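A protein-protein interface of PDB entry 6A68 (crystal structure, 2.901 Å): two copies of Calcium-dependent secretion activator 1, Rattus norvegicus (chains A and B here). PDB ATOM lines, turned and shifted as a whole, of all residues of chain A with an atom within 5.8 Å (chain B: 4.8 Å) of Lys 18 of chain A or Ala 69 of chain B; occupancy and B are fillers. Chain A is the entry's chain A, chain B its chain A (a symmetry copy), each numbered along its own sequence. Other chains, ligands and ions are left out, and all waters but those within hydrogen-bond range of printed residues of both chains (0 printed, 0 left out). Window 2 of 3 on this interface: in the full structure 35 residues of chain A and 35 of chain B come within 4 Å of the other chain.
The backbone carbonyl oxygen of Pro 15 of chain A lies close to the side-chain amide oxygen of Gln 73 of chain B (3.3 Å). O of Asp 65 of chain B sits at hydrogen-bond distance from OG1 of Thr 22 of chain A, 3.2 Å away.
O of Lys 18 of chain A is in hydrogen-bond range of OG1 of Thr 22 of chain A. The backbone carbonyl oxygen (O) of Ala 69 of chain B lies close to the side-chain amide oxygen (OE1) of Gln 73 of chain B (3.2 Å).
Among the printed residues, merely in contact across the chains: Lys 18 of chain A with Ala 69 of chain B, Pro 15 of chain A with Val 72 of chain B and Thr 22 of chain A with Ala 69 of chain B.
Lys 18 of chain A touches just one residue of chain B: Ala 69. Ala 69 of chain B touches just these residues of chain A: Lys 18 and Thr 22. Of the printed residues of chain B, Pro 15 of chain A touches Val 72 and Gln 73. Of the printed residues of chain A, Asp 65 of chain B touches Thr 22 (3.2 Å). Printed residues of chain B within 4 Å of Thr 22 of chain A: Asp 65 and Ala 69.
Of the 9 printed residues of chain B, 4 touch a printed residue of chain A. Of the 10 printed residues of chain A, 3 touch a printed residue of chain B. Hydrophobic or aromatic side chains of chain A that line the printed part of chain B: Pro 15. Along chain A the printed residues that touch a printed residue of chain B span positions 15 to 22. Among the printed residues, no Asp or Glu carboxylate lies within 4 Å of a Lys or Arg side-chain nitrogen of the other chain.
No position is printed for both chains. Of the 5 pairs that touch across the chains among the printed residues, none has its exchanged pair printed and touching as well.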
ATOM      1  N   ILE A  13      29.021 -13.987  24.354  1.00  0.00           N
ATOM      2  CA  ILE A  13      29.049 -12.531  24.450  1.00  0.00           C
ATOM      3  C   ILE A  13      27.806 -12.095  25.218  1.00  0.00           C
ATOM      4  O   ILE A  13      26.710 -12.022  24.649  1.00  0.00           O
ATOM      5  CB  ILE A  13      29.108 -11.862  23.072  1.00  0.00           C
ATOM      6  CG1 ILE A  13      28.302 -12.675  22.052  1.00  0.00           C
ATOM      7  N   THR A  14      27.972 -11.808  26.514  1.00  0.00           N
ATOM      8  CA  THR A  14      26.931 -11.182  27.326  1.00  0.00           C
ATOM      9  C   THR A  14      26.419  -9.930  26.624  1.00  0.00           C
ATOM     10  O   THR A  14      27.132  -8.921  26.577  1.00  0.00           O
ATOM     11  CB  THR A  14      27.469 -10.794  28.709  1.00  0.00           C
ATOM     12  OG1 THR A  14      28.435 -11.759  29.156  1.00  0.00           O
ATOM     13  CG2 THR A  14      26.330 -10.670  29.720  1.00  0.00           C
ATOM     14  N   PRO A  15      25.201  -9.933  26.079  1.00  0.00           N
ATOM     15  CA  PRO A  15      24.727  -8.749  25.336  1.00  0.00           C
ATOM     16  C   PRO A  15      24.599  -7.492  26.194  1.00  0.00           C
ATOM     17  O   PRO A  15      24.361  -6.408  25.645  1.00  0.00           O
ATOM     18  CB  PRO A  15      23.365  -9.195  24.792  1.00  0.00           C
ATOM     19  CG  PRO A  15      22.915 -10.240  25.751  1.00  0.00           C
ATOM     20  CD  PRO A  15      24.152 -10.950  26.238  1.00  0.00           C
ATOM     21  N   ALA A  16      24.735  -7.608  27.514  1.00  0.00           N
ATOM     22  CA  ALA A  16      24.846  -6.468  28.413  1.00  0.00           C
ATOM     23  C   ALA A  16      26.293  -6.145  28.754  1.00  0.00           C
ATOM     24  O   ALA A  16      26.546  -5.199  29.508  1.00  0.00           O
ATOM     25  CB  ALA A  16      24.053  -6.722  29.701  1.00  0.00           C
ATOM     26  N   LYS A  17      27.239  -6.935  28.250  1.00  0.00           N
ATOM     27  CA  LYS A  17      28.639  -6.543  28.178  1.00  0.00           C
ATOM     28  C   LYS A  17      28.988  -5.964  26.816  1.00  0.00           C
ATOM     29  O   LYS A  17      29.682  -4.949  26.740  1.00  0.00           O
ATOM     30  CB  LYS A  17      29.545  -7.739  28.480  1.00  0.00           C
ATOM     31  CG  LYS A  17      30.987  -7.401  28.848  1.00  0.00           C
ATOM     32  CD  LYS A  17      31.868  -8.654  28.781  1.00  0.00           C
ATOM     33  CE  LYS A  17      32.985  -8.553  27.731  1.00  0.00           C
ATOM     34  NZ  LYS A  17      34.309  -8.155  28.311  1.00  0.00           N
ATOM     35  N   LYS A  18      28.486  -6.558  25.732  1.00  0.00           N
ATOM     36  CA  LYS A  18      28.684  -5.955  24.419  1.00  0.00           C
ATOM     37  C   LYS A  18      27.988  -4.612  24.294  1.00  0.00           C
ATOM     38  O   LYS A  18      28.146  -3.949  23.266  1.00  0.00           O
ATOM     39  CB  LYS A  18      28.197  -6.882  23.303  1.00  0.00           C
ATOM     40  N   LEU A  19      27.212  -4.199  25.293  1.00  0.00           N
ATOM     41  CA  LEU A  19      26.744  -2.824  25.363  1.00  0.00           C
ATOM     42  C   LEU A  19      27.551  -2.003  26.358  1.00  0.00           C
ATOM     43  O   LEU A  19      28.083  -0.955  25.995  1.00  0.00           O
ATOM     44  CB  LEU A  19      25.259  -2.771  25.726  1.00  0.00           C
ATOM     45  CG  LEU A  19      24.631  -1.389  25.550  1.00  0.00           C
ATOM     46  CD1 LEU A  19      24.249  -1.162  24.097  1.00  0.00           C
ATOM     47  CD2 LEU A  19      23.427  -1.234  26.453  1.00  0.00           C
ATOM     48  N   GLU A  20      27.668  -2.471  27.602  1.00  0.00           N
ATOM     49  CA  GLU A  20      28.490  -1.771  28.583  1.00  0.00           C
ATOM     50  C   GLU A  20      29.898  -1.525  28.054  1.00  0.00           C
ATOM     51  O   GLU A  20      30.539  -0.531  28.419  1.00  0.00           O
ATOM     52  CB  GLU A  20      28.507  -2.562  29.902  1.00  0.00           C
ATOM     53  CG  GLU A  20      29.878  -2.797  30.528  1.00  0.00           C
ATOM     54  CD  GLU A  20      30.551  -4.058  30.014  1.00  0.00           C
ATOM     55  N   ASP A  21      30.383  -2.388  27.160  1.00  0.00           N
ATOM     56  CA  ASP A  21      31.695  -2.165  26.566  1.00  0.00           C
ATOM     57  C   ASP A  21      31.629  -1.100  25.479  1.00  0.00           C
ATOM     58  O   ASP A  21      32.457  -0.185  25.453  1.00  0.00           O
ATOM     59  CB  ASP A  21      32.265  -3.476  26.016  1.00  0.00           C
ATOM     60  CG  ASP A  21      33.054  -4.256  27.061  1.00  0.00           C
ATOM     61  OD1 ASP A  21      33.227  -3.747  28.195  1.00  0.00           O
ATOM     62  OD2 ASP A  21      33.512  -5.374  26.743  1.00  0.00           O
ATOM     63  N   THR A  22      30.646  -1.201  24.580  1.00  0.00           N
ATOM     64  CA  THR A  22      30.454  -0.154  23.580  1.00  0.00           C
ATOM     65  C   THR A  22      30.289   1.221  24.224  1.00  0.00           C
ATOM     66  O   THR A  22      30.750   2.223  23.666  1.00  0.00           O
ATOM     67  CB  THR A  22      29.247  -0.488  22.705  1.00  0.00           C
ATOM     68  OG1 THR A  22      29.546  -1.646  21.917  1.00  0.00           O
ATOM     69  CG2 THR A  22      28.906   0.663  21.765  1.00  0.00           C
ATOM     70  N   ASP B  65      31.348  -1.178  15.979  1.00  0.00           N
ATOM     71  CA  ASP B  65      31.140  -1.693  17.330  1.00  0.00           C
ATOM     72  C   ASP B  65      29.758  -1.350  17.871  1.00  0.00           C
ATOM     73  O   ASP B  65      29.280  -2.020  18.792  1.00  0.00           O
ATOM     74  CB  ASP B  65      32.193  -1.147  18.295  1.00  0.00           C
ATOM     75  CG  ASP B  65      33.514  -1.877  18.198  1.00  0.00           C
ATOM     76  OD1 ASP B  65      33.985  -2.116  17.066  1.00  0.00           O
ATOM     77  OD2 ASP B  65      34.091  -2.201  19.260  1.00  0.00           O
ATOM     78  N   MET B  66      29.118  -0.316  17.344  1.00  0.00           N
ATOM     79  CA  MET B  66      27.821   0.111  17.840  1.00  0.00           C
ATOM     80  C   MET B  66      26.729  -0.623  17.084  1.00  0.00           C
ATOM     81  O   MET B  66      25.836  -1.209  17.689  1.00  0.00           O
ATOM     82  CB  MET B  66      27.662   1.619  17.691  1.00  0.00           C
ATOM     83  CG  MET B  66      26.340   2.145  18.183  1.00  0.00           C
ATOM     84  SD  MET B  66      26.065   4.046  17.813  1.00  0.00           S
ATOM     85  CE  MET B  66      25.981   4.052  15.861  1.00  0.00           C
ATOM     86  N   ASP B  67      26.819  -0.592  15.751  1.00  0.00           N
ATOM     87  CA  ASP B  67      25.935  -1.402  14.924  1.00  0.00           C
ATOM     88  C   ASP B  67      25.931  -2.857  15.368  1.00  0.00           C
ATOM     89  O   ASP B  67      24.897  -3.528  15.295  1.00  0.00           O
ATOM     90  CB  ASP B  67      26.358  -1.309  13.461  1.00  0.00           C
ATOM     91  CG  ASP B  67      26.107   0.059  12.875  1.00  0.00           C
ATOM     92  OD1 ASP B  67      25.766   0.974  13.652  1.00  0.00           O
ATOM     93  OD2 ASP B  67      26.249   0.226  11.643  1.00  0.00           O
ATOM     94  N   ALA B  68      27.070  -3.358  15.839  1.00  0.00           N
ATOM     95  CA  ALA B  68      27.146  -4.744  16.277  1.00  0.00           C
ATOM     96  C   ALA B  68      26.480  -4.936  17.627  1.00  0.00           C
ATOM     97  O   ALA B  68      25.821  -5.957  17.854  1.00  0.00           O
ATOM     98  CB  ALA B  68      28.602  -5.205  16.339  1.00  0.00           C
ATOM     99  N   ALA B  69      26.643  -3.980  18.542  1.00  0.00           N
ATOM    100  CA  ALA B  69      25.976  -4.098  19.830  1.00  0.00           C
ATOM    101  C   ALA B  69      24.465  -3.928  19.732  1.00  0.00           C
ATOM    102  O   ALA B  69      23.763  -4.245  20.698  1.00  0.00           O
ATOM    103  CB  ALA B  69      26.535  -3.082  20.814  1.00  0.00           C
ATOM    104  N   LEU B  70      23.943  -3.445  18.606  1.00  0.00           N
ATOM    105  CA  LEU B  70      22.511  -3.224  18.475  1.00  0.00           C
ATOM    106  C   LEU B  70      21.811  -4.320  17.687  1.00  0.00           C
ATOM    107  O   LEU B  70      20.630  -4.174  17.356  1.00  0.00           O
ATOM    108  CB  LEU B  70      22.225  -1.853  17.863  1.00  0.00           C
ATOM    109  CG  LEU B  70      22.443  -0.714  18.871  1.00  0.00           C
ATOM    110  CD1 LEU B  70      21.656   0.526  18.496  1.00  0.00           C
ATOM    111  CD2 LEU B  70      22.119  -1.133  20.304  1.00  0.00           C
ATOM    112  N   GLU B  71      22.507  -5.417  17.385  1.00  0.00           N
ATOM    113  CA  GLU B  71      21.852  -6.650  16.975  1.00  0.00           C
ATOM    114  C   GLU B  71      21.891  -7.716  18.057  1.00  0.00           C
ATOM    115  O   GLU B  71      21.001  -8.568  18.091  1.00  0.00           O
ATOM    116  CB  GLU B  71      22.479  -7.203  15.684  1.00  0.00           C
ATOM    117  CG  GLU B  71      22.993  -6.138  14.721  1.00  0.00           C
ATOM    118  CD  GLU B  71      21.944  -5.092  14.359  1.00  0.00           C
ATOM    119  OE1 GLU B  71      22.317  -3.915  14.139  1.00  0.00           O
ATOM    120  OE2 GLU B  71      20.747  -5.447  14.283  1.00  0.00           O
ATOM    121  N   VAL B  72      22.864  -7.660  18.965  1.00  0.00           N
ATOM    122  CA  VAL B  72      22.892  -8.501  20.159  1.00  0.00           C
ATOM    123  C   VAL B  72      21.784  -8.072  21.122  1.00  0.00           C
ATOM    124  O   VAL B  72      21.686  -8.578  22.249  1.00  0.00           O
ATOM    125  CB  VAL B  72      24.279  -8.443  20.835  1.00  0.00           C
ATOM    126  CG1 VAL B  72      24.394  -7.233  21.775  1.00  0.00           C
ATOM    127  CG2 VAL B  72      24.605  -9.752  21.568  1.00  0.00           C
ATOM    128  N   GLN B  73      20.929  -7.135  20.681  1.00  0.00           N
ATOM    129  CA  GLN B  73      19.897  -6.571  21.545  1.00  0.00           C
ATOM    130  C   GLN B  73      18.591  -7.337  21.385  1.00  0.00           C
ATOM    131  O   GLN B  73      18.084  -7.451  20.261  1.00  0.00           O
ATOM    132  CB  GLN B  73      19.668  -5.097  21.226  1.00  0.00           C
ATOM    133  CG  GLN B  73      20.740  -4.186  21.785  1.00  0.00           C
ATOM    134  CD  GLN B  73      21.135  -4.549  23.212  1.00  0.00           C
ATOM    135  OE1 GLN B  73      22.239  -5.041  23.455  1.00  0.00           O
ATOM    136  NE2 GLN B  73      20.234  -4.304  24.161  1.00  0.00           N
